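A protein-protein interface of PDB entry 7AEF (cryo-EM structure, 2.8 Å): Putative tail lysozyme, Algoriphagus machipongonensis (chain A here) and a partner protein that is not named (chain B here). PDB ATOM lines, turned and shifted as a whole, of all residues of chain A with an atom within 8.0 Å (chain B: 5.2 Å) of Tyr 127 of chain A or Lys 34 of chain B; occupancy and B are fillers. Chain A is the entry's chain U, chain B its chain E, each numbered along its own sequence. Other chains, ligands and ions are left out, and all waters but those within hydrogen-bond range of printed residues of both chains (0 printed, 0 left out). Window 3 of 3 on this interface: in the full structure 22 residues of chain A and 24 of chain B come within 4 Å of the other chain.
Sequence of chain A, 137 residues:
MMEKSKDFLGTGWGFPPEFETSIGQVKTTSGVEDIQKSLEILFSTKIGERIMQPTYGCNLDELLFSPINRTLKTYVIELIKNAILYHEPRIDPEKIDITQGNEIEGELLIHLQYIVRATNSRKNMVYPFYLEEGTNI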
ATOM      1  N   ASP A   7     -14.226 -28.715  16.437  1.00  0.00           N
ATOM      2  CA  ASP A   7     -14.504 -28.582  17.871  1.00  0.00           C
ATOM      3  C   ASP A   7     -14.340 -27.148  18.362  1.00  0.00           C
ATOM      4  O   ASP A   7     -14.618 -26.885  19.534  1.00  0.00           O
ATOM      5  CB  ASP A   7     -13.545 -29.500  18.606  1.00  0.00           C
ATOM      6  CG  ASP A   7     -13.828 -30.919  18.354  1.00  0.00           C
ATOM      7  OD1 ASP A   7     -13.211 -31.703  19.063  1.00  0.00           O
ATOM      8  OD2 ASP A   7     -14.749 -31.218  17.545  1.00  0.00           O
ATOM      9  N   PHE A   8     -13.885 -26.216  17.510  1.00  0.00           N
ATOM     10  CA  PHE A   8     -13.765 -24.825  17.945  1.00  0.00           C
ATOM     11  C   PHE A   8     -15.002 -24.005  17.647  1.00  0.00           C
ATOM     12  O   PHE A   8     -15.013 -22.800  17.917  1.00  0.00           O
ATOM     13  CB  PHE A   8     -12.501 -24.113  17.389  1.00  0.00           C
ATOM     14  CG  PHE A   8     -12.385 -24.009  15.898  1.00  0.00           C
ATOM     15  CD1 PHE A   8     -13.052 -23.029  15.175  1.00  0.00           C
ATOM     16  CD2 PHE A   8     -11.500 -24.821  15.236  1.00  0.00           C
ATOM     17  CE1 PHE A   8     -12.890 -22.926  13.829  1.00  0.00           C
ATOM     18  CE2 PHE A   8     -11.331 -24.709  13.886  1.00  0.00           C
ATOM     19  CZ  PHE A   8     -12.030 -23.763  13.185  1.00  0.00           C
ATOM     20  N   GLY A  10     -17.784 -25.100  18.963  1.00  0.00           N
ATOM     21  CA  GLY A  10     -18.305 -25.310  20.295  1.00  0.00           C
ATOM     22  C   GLY A  10     -19.705 -25.894  20.366  1.00  0.00           C
ATOM     23  O   GLY A  10     -20.357 -26.190  19.362  1.00  0.00           O
ATOM     24  N   THR A  11     -20.135 -26.105  21.628  1.00  0.00           N
ATOM     25  CA  THR A  11     -21.405 -26.703  22.086  1.00  0.00           C
ATOM     26  C   THR A  11     -22.099 -25.905  23.202  1.00  0.00           C
ATOM     27  O   THR A  11     -21.442 -25.545  24.165  1.00  0.00           O
ATOM     28  CB  THR A  11     -21.135 -28.094  22.689  1.00  0.00           C
ATOM     29  OG1 THR A  11     -20.335 -28.873  21.805  1.00  0.00           O
ATOM     30  CG2 THR A  11     -22.413 -28.838  22.963  1.00  0.00           C
ATOM     31  N   ASN A 124     -13.242 -15.750  19.646  1.00  0.00           N
ATOM     32  CA  ASN A 124     -14.159 -16.871  19.854  1.00  0.00           C
ATOM     33  C   ASN A 124     -13.931 -17.578  21.196  1.00  0.00           C
ATOM     34  O   ASN A 124     -13.007 -18.374  21.345  1.00  0.00           O
ATOM     35  CB  ASN A 124     -13.992 -17.826  18.692  1.00  0.00           C
ATOM     36  CG  ASN A 124     -14.926 -18.944  18.743  1.00  0.00           C
ATOM     37  OD1 ASN A 124     -16.033 -18.836  19.265  1.00  0.00           O
ATOM     38  ND2 ASN A 124     -14.499 -20.053  18.189  1.00  0.00           N
ATOM     39  N   MET A 125     -14.758 -17.311  22.194  1.00  0.00           N
ATOM     40  CA  MET A 125     -14.512 -17.905  23.508  1.00  0.00           C
ATOM     41  C   MET A 125     -15.024 -19.343  23.687  1.00  0.00           C
ATOM     42  O   MET A 125     -15.993 -19.613  24.366  1.00  0.00           O
ATOM     43  CB  MET A 125     -15.062 -16.987  24.586  1.00  0.00           C
ATOM     44  CG  MET A 125     -14.880 -17.534  25.986  1.00  0.00           C
ATOM     45  SD  MET A 125     -14.647 -16.373  27.293  1.00  0.00           S
ATOM     46  CE  MET A 125     -13.270 -15.429  26.685  1.00  0.00           C
ATOM     47  N   VAL A 126     -14.324 -20.286  23.077  1.00  0.00           N
ATOM     48  CA  VAL A 126     -14.600 -21.718  23.179  1.00  0.00           C
ATOM     49  C   VAL A 126     -13.492 -22.346  24.022  1.00  0.00           C
ATOM     50  O   VAL A 126     -12.306 -22.142  23.742  1.00  0.00           O
ATOM     51  CB  VAL A 126     -14.731 -22.335  21.776  1.00  0.00           C
ATOM     52  CG1 VAL A 126     -14.963 -23.822  21.824  1.00  0.00           C
ATOM     53  CG2 VAL A 126     -15.897 -21.677  21.102  1.00  0.00           C
ATOM     54  N   TYR A 127     -13.882 -23.087  25.068  1.00  0.00           N
ATOM     55  CA  TYR A 127     -13.007 -23.444  26.193  1.00  0.00           C
ATOM     56  C   TYR A 127     -11.592 -23.975  25.909  1.00  0.00           C
ATOM     57  O   TYR A 127     -10.643 -23.413  26.459  1.00  0.00           O
ATOM     58  CB  TYR A 127     -13.722 -24.416  27.147  1.00  0.00           C
ATOM     59  CG  TYR A 127     -12.736 -25.104  28.049  1.00  0.00           C
ATOM     60  CD1 TYR A 127     -12.062 -24.398  29.037  1.00  0.00           C
ATOM     61  CD2 TYR A 127     -12.479 -26.459  27.917  1.00  0.00           C
ATOM     62  CE1 TYR A 127     -11.149 -25.010  29.812  1.00  0.00           C
ATOM     63  CE2 TYR A 127     -11.578 -27.070  28.708  1.00  0.00           C
ATOM     64  CZ  TYR A 127     -10.918 -26.349  29.653  1.00  0.00           C
ATOM     65  OH  TYR A 127     -10.009 -26.982  30.452  1.00  0.00           O
ATOM     66  N   PRO A 128     -11.349 -25.034  25.151  1.00  0.00           N
ATOM     67  CA  PRO A 128      -9.971 -25.498  25.039  1.00  0.00           C
ATOM     68  C   PRO A 128      -9.145 -24.715  24.027  1.00  0.00           C
ATOM     69  O   PRO A 128      -8.022 -25.114  23.726  1.00  0.00           O
ATOM     70  CB  PRO A 128     -10.170 -26.959  24.646  1.00  0.00           C
ATOM     71  CG  PRO A 128     -11.423 -26.932  23.837  1.00  0.00           C
ATOM     72  CD  PRO A 128     -12.279 -25.849  24.357  1.00  0.00           C
ATOM     73  N   PHE A 129      -9.649 -23.592  23.513  1.00  0.00           N
ATOM     74  CA  PHE A 129      -8.945 -22.832  22.492  1.00  0.00           C
ATOM     75  C   PHE A 129      -8.583 -21.433  22.926  1.00  0.00           C
ATOM     76  O   PHE A 129      -7.424 -21.046  22.766  1.00  0.00           O
ATOM     77  CB  PHE A 129      -9.768 -22.734  21.223  1.00  0.00           C
ATOM     78  CG  PHE A 129     -10.037 -24.027  20.628  1.00  0.00           C
ATOM     79  CD1 PHE A 129     -11.208 -24.671  20.906  1.00  0.00           C
ATOM     80  CD2 PHE A 129      -9.115 -24.622  19.806  1.00  0.00           C
ATOM     81  CE1 PHE A 129     -11.460 -25.885  20.379  1.00  0.00           C
ATOM     82  CE2 PHE A 129      -9.370 -25.845  19.266  1.00  0.00           C
ATOM     83  CZ  PHE A 129     -10.548 -26.477  19.552  1.00  0.00           C
ATOM     84  N   TYR A 130      -9.537 -20.665  23.478  1.00  0.00           N
ATOM     85  CA  TYR A 130      -9.256 -19.264  23.789  1.00  0.00           C
ATOM     86  C   TYR A 130      -8.101 -19.109  24.766  1.00  0.00           C
ATOM     87  O   TYR A 130      -7.392 -18.106  24.708  1.00  0.00           O
ATOM     88  CB  TYR A 130     -10.502 -18.542  24.321  1.00  0.00           C
ATOM     89  CG  TYR A 130     -10.934 -18.849  25.739  1.00  0.00           C
ATOM     90  CD1 TYR A 130     -10.345 -18.233  26.835  1.00  0.00           C
ATOM     91  CD2 TYR A 130     -11.980 -19.698  25.975  1.00  0.00           C
ATOM     92  CE1 TYR A 130     -10.737 -18.502  28.087  1.00  0.00           C
ATOM     93  CE2 TYR A 130     -12.396 -19.957  27.242  1.00  0.00           C
ATOM     94  CZ  TYR A 130     -11.772 -19.361  28.292  1.00  0.00           C
ATOM     95  OH  TYR A 130     -12.191 -19.625  29.563  1.00  0.00           O
ATOM     96  N   LEU A 131      -7.840 -20.125  25.580  1.00  0.00           N
ATOM     97  CA  LEU A 131      -6.783 -20.040  26.575  1.00  0.00           C
ATOM     98  C   LEU A 131      -5.427 -19.739  25.968  1.00  0.00           C
ATOM     99  O   LEU A 131      -4.627 -19.024  26.569  1.00  0.00           O
ATOM    100  CB  LEU A 131      -6.673 -21.340  27.339  1.00  0.00           C
ATOM    101  CG  LEU A 131      -7.827 -21.776  28.216  1.00  0.00           C
ATOM    102  CD1 LEU A 131      -7.451 -23.106  28.825  1.00  0.00           C
ATOM    103  CD2 LEU A 131      -8.113 -20.744  29.286  1.00  0.00           C
ATOM    104  N   GLU A 132      -5.139 -20.288  24.794  1.00  0.00           N
ATOM    105  CA  GLU A 132      -3.869 -19.972  24.200  1.00  0.00           C
ATOM    106  C   GLU A 132      -4.051 -19.158  22.907  1.00  0.00           C
ATOM    107  O   GLU A 132      -3.157 -18.413  22.536  1.00  0.00           O
ATOM    108  CB  GLU A 132      -3.126 -21.246  23.834  1.00  0.00           C
ATOM    109  CG  GLU A 132      -1.637 -21.121  23.941  1.00  0.00           C
ATOM    110  CD  GLU A 132      -1.187 -20.934  25.384  1.00  0.00           C
ATOM    111  OE1 GLU A 132      -1.602 -21.786  26.217  1.00  0.00           O
ATOM    112  OE2 GLU A 132      -0.443 -19.994  25.691  1.00  0.00           O
ATOM    113  N   ILE B  30     -17.393 -18.882  35.892  1.00  0.00           N
ATOM    114  CA  ILE B  30     -16.891 -19.588  34.726  1.00  0.00           C
ATOM    115  C   ILE B  30     -15.848 -20.624  35.104  1.00  0.00           C
ATOM    116  O   ILE B  30     -15.840 -21.719  34.535  1.00  0.00           O
ATOM    117  CB  ILE B  30     -16.377 -18.608  33.665  1.00  0.00           C
ATOM    118  CG1 ILE B  30     -17.599 -17.865  33.117  1.00  0.00           C
ATOM    119  CG2 ILE B  30     -15.672 -19.380  32.541  1.00  0.00           C
ATOM    120  CD1 ILE B  30     -17.313 -16.671  32.284  1.00  0.00           C
ATOM    121  N   ARG B  31     -14.959 -20.307  36.048  1.00  0.00           N
ATOM    122  CA  ARG B  31     -13.981 -21.297  36.485  1.00  0.00           C
ATOM    123  C   ARG B  31     -14.655 -22.556  37.006  1.00  0.00           C
ATOM    124  O   ARG B  31     -14.267 -23.665  36.628  1.00  0.00           O
ATOM    125  CB  ARG B  31     -13.080 -20.722  37.567  1.00  0.00           C
ATOM    126  CG  ARG B  31     -12.038 -21.692  38.067  1.00  0.00           C
ATOM    127  CD  ARG B  31     -11.075 -21.068  39.045  1.00  0.00           C
ATOM    128  NE  ARG B  31     -11.661 -20.659  40.333  1.00  0.00           N
ATOM    129  CZ  ARG B  31     -11.947 -21.471  41.365  1.00  0.00           C
ATOM    130  NH1 ARG B  31     -11.761 -22.787  41.311  1.00  0.00           N
ATOM    131  NH2 ARG B  31     -12.429 -20.953  42.483  1.00  0.00           N
ATOM    132  N   TYR B  32     -15.704 -22.403  37.811  1.00  0.00           N
ATOM    133  CA  TYR B  32     -16.405 -23.569  38.328  1.00  0.00           C
ATOM    134  C   TYR B  32     -17.058 -24.372  37.217  1.00  0.00           C
ATOM    135  O   TYR B  32     -17.008 -25.603  37.245  1.00  0.00           O
ATOM    136  CB  TYR B  32     -17.465 -23.165  39.341  1.00  0.00           C
ATOM    137  CG  TYR B  32     -16.919 -22.622  40.616  1.00  0.00           C
ATOM    138  CD1 TYR B  32     -17.333 -21.400  41.081  1.00  0.00           C
ATOM    139  CD2 TYR B  32     -16.002 -23.326  41.349  1.00  0.00           C
ATOM    140  CE1 TYR B  32     -16.838 -20.881  42.227  1.00  0.00           C
ATOM    141  CE2 TYR B  32     -15.505 -22.811  42.505  1.00  0.00           C
ATOM    142  CZ  TYR B  32     -15.925 -21.592  42.937  1.00  0.00           C
ATOM    143  OH  TYR B  32     -15.426 -21.082  44.099  1.00  0.00           O
ATOM    144  N   ILE B  33     -17.631 -23.690  36.219  1.00  0.00           N
ATOM    145  CA  ILE B  33     -18.275 -24.374  35.101  1.00  0.00           C
ATOM    146  C   ILE B  33     -17.291 -25.249  34.359  1.00  0.00           C
ATOM    147  O   ILE B  33     -17.604 -26.392  34.038  1.00  0.00           O
ATOM    148  CB  ILE B  33     -18.914 -23.383  34.120  1.00  0.00           C
ATOM    149  CG1 ILE B  33     -20.115 -22.715  34.769  1.00  0.00           C
ATOM    150  CG2 ILE B  33     -19.310 -24.098  32.801  1.00  0.00           C
ATOM    151  CD1 ILE B  33     -20.632 -21.505  34.036  1.00  0.00           C
ATOM    152  N   LYS B  34     -16.103 -24.738  34.057  1.00  0.00           N
ATOM    153  CA  LYS B  34     -15.139 -25.559  33.335  1.00  0.00           C
ATOM    154  C   LYS B  34     -14.730 -26.772  34.116  1.00  0.00           C
ATOM    155  O   LYS B  34     -14.604 -27.849  33.553  1.00  0.00           O
ATOM    156  CB  LYS B  34     -13.868 -24.807  33.045  1.00  0.00           C
ATOM    157  CG  LYS B  34     -13.994 -23.704  32.069  1.00  0.00           C
ATOM    158  CD  LYS B  34     -12.623 -23.186  31.700  1.00  0.00           C
ATOM    159  CE  LYS B  34     -11.957 -22.493  32.869  1.00  0.00           C
ATOM    160  NZ  LYS B  34     -10.653 -21.855  32.542  1.00  0.00           N
ATOM    161  N   GLU B  35     -14.496 -26.607  35.404  1.00  0.00           N
ATOM    162  CA  GLU B  35     -14.049 -27.721  36.225  1.00  0.00           C
ATOM    163  C   GLU B  35     -15.075 -28.836  36.299  1.00  0.00           C
ATOM    164  O   GLU B  35     -14.719 -30.015  36.293  1.00  0.00           O
ATOM    165  CB  GLU B  35     -13.740 -27.218  37.624  1.00  0.00           C
ATOM    166  CG  GLU B  35     -12.511 -26.335  37.691  1.00  0.00           C
ATOM    167  CD  GLU B  35     -12.319 -25.699  39.038  1.00  0.00           C
ATOM    168  OE1 GLU B  35     -13.135 -25.946  39.915  1.00  0.00           O
ATOM    169  OE2 GLU B  35     -11.364 -24.939  39.211  1.00  0.00           O
ATOM    170  N   LEU B  36     -16.346 -28.484  36.348  1.00  0.00           N
ATOM    171  CA  LEU B  36     -17.405 -29.468  36.474  1.00  0.00           C
ATOM    172  C   LEU B  36     -17.974 -30.005  35.164  1.00  0.00           C
ATOM    173  O   LEU B  36     -18.293 -31.192  35.087  1.00  0.00           O
ATOM    174  CB  LEU B  36     -18.548 -28.854  37.259  1.00  0.00           C
ATOM    175  CG  LEU B  36     -18.264 -28.444  38.694  1.00  0.00           C
ATOM    176  CD1 LEU B  36     -19.434 -27.672  39.203  1.00  0.00           C
ATOM    177  CD2 LEU B  36     -18.039 -29.660  39.560  1.00  0.00           C
ATOM    178  N   GLY B  37     -18.171 -29.165  34.147  1.00  0.00           N
ATOM    179  CA  GLY B  37     -18.875 -29.613  32.957  1.00  0.00           C
ATOM    180  C   GLY B  37     -18.269 -29.392  31.580  1.00  0.00           C
ATOM    181  O   GLY B  37     -18.996 -29.535  30.594  1.00  0.00           O
ATOM    182  N   SER B  38     -16.953 -29.155  31.462  1.00  0.00           N
ATOM    183  CA  SER B  38     -16.345 -28.838  30.169  1.00  0.00           C
ATOM    184  C   SER B  38     -16.443 -29.980  29.146  1.00  0.00           C
ATOM    185  O   SER B  38     -16.226 -29.747  27.958  1.00  0.00           O
ATOM    186  CB  SER B  38     -14.875 -28.528  30.319  1.00  0.00           C
ATOM    187  OG  SER B  38     -14.167 -29.630  30.806  1.00  0.00           O
ATOM    188  N   THR B  42     -18.903 -26.254  26.293  1.00  0.00           N
ATOM    189  CA  THR B  42     -17.650 -25.589  25.948  1.00  0.00           C
ATOM    190  C   THR B  42     -17.808 -24.191  25.352  1.00  0.00           C
ATOM    191  O   THR B  42     -16.844 -23.428  25.320  1.00  0.00           O
ATOM    192  CB  THR B  42     -16.866 -26.440  24.948  1.00  0.00           C
ATOM    193  OG1 THR B  42     -17.635 -26.576  23.753  1.00  0.00           O
ATOM    194  CG2 THR B  42     -16.621 -27.792  25.520  1.00  0.00           C
ATOM    195  N   ASP B  43     -18.977 -23.838  24.872  1.00  0.00           N
ATOM    196  CA  ASP B  43     -19.224 -22.557  24.235  1.00  0.00           C
ATOM    197  C   ASP B  43     -19.541 -21.535  25.321  1.00  0.00           C
ATOM    198  O   ASP B  43     -20.660 -21.511  25.810  1.00  0.00           O
ATOM    199  CB  ASP B  43     -20.396 -22.768  23.281  1.00  0.00           C
ATOM    200  CG  ASP B  43     -20.926 -21.511  22.662  1.00  0.00           C
ATOM    201  OD1 ASP B  43     -20.565 -20.398  23.013  1.00  0.00           O
ATOM    202  OD2 ASP B  43     -21.777 -21.613  21.779  1.00  0.00           O
ATOM    203  N   TYR B  44     -18.636 -20.599  25.591  1.00  0.00           N
ATOM    204  CA  TYR B  44     -18.885 -19.624  26.649  1.00  0.00           C
ATOM    205  C   TYR B  44     -19.060 -18.221  26.096  1.00  0.00           C
ATOM    206  O   TYR B  44     -18.783 -17.239  26.782  1.00  0.00           O
ATOM    207  CB  TYR B  44     -17.790 -19.643  27.715  1.00  0.00           C
ATOM    208  CG  TYR B  44     -17.553 -21.004  28.302  1.00  0.00           C
ATOM    209  CD1 TYR B  44     -16.282 -21.458  28.439  1.00  0.00           C
ATOM    210  CD2 TYR B  44     -18.595 -21.841  28.663  1.00  0.00           C
ATOM    211  CE1 TYR B  44     -16.033 -22.690  28.916  1.00  0.00           C
ATOM    212  CE2 TYR B  44     -18.344 -23.085  29.136  1.00  0.00           C
ATOM    213  CZ  TYR B  44     -17.058 -23.503  29.260  1.00  0.00           C
ATOM    214  OH  TYR B  44     -16.772 -24.760  29.703  1.00  0.00           O
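Of the 13 printed residues of chain A, 5 touch a printed residue of chain B. Printed residues of chain B that touch a printed residue of chain A: Lys 34, Ser 38, Thr 42, Asp 43 and Tyr 44. Among the printed residues, no Asp or Glu carboxylate lies within 4 Å of a Lys or Arg side-chain nitrogen of the other chain.
The side-chain hydroxyl of Thr 42 of chain B sits at hydrogen-bond distance from the backbone NH of Thr 11 of chain A (3.3 Å). O of Thr 42 of chain B is in hydrogen-bond range of N of Tyr 127 of chain A. The backbone NH (N) of Asp 43 of chain B lies within hydrogen-bond range of the backbone carbonyl oxygen (O) of Thr 11 of chain A. The backbone NH (N) of Tyr 44 of chain B lies within hydrogen-bond range of the backbone carbonyl oxygen (O) of Met 125 of chain A.
Tyr 127 of chain A touches four residues of chain B. Lys 34 of chain B touches one residue of chain A. Printed residues of chain A within 4 Å of Asp 43 of chain B: Thr 11. Of the printed residues of chain A, Thr 42 of chain B touches Gly 10, Thr 11, Val 126 and Tyr 127. Of the printed residues of chain B, Thr 11 of chain A touches Thr 42 (3.3 Å) and Asp 43 (3.1 Å). Of the printed residues of chain B, Gly 10 of chain A touches Thr 42 (3.7 Å). Of the printed residues of chain A, Ser 38 of chain B touches Tyr 127. The nearest printed residue of chain B that does not touch Tyr 127 of chain A is Asp 43 of chain B (5.2 Å). The nearest printed residue of chain B that does not touch Met 125 of chain A is Thr 42 of chain B (4.02 Å).
The side-chain hydroxyl (OG) of Ser 38 of chain B is in hydrogen-bond range of the backbone carbonyl oxygen (O) of Lys 34 of chain B.
Among the printed residues, merely in contact across the chains: Tyr 127 of chain A with Lys 34 of chain B (3.0 Å), Tyr 127 of chain A with Tyr 44 of chain B (3.4 Å), Val 126 of chain A with Thr 42 of chain B (3.5 Å), Gly 10 of chain A with Thr 42 of chain B (3.7 Å) and Tyr 127 of chain A with Ser 38 of chain B (3.9 Å).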
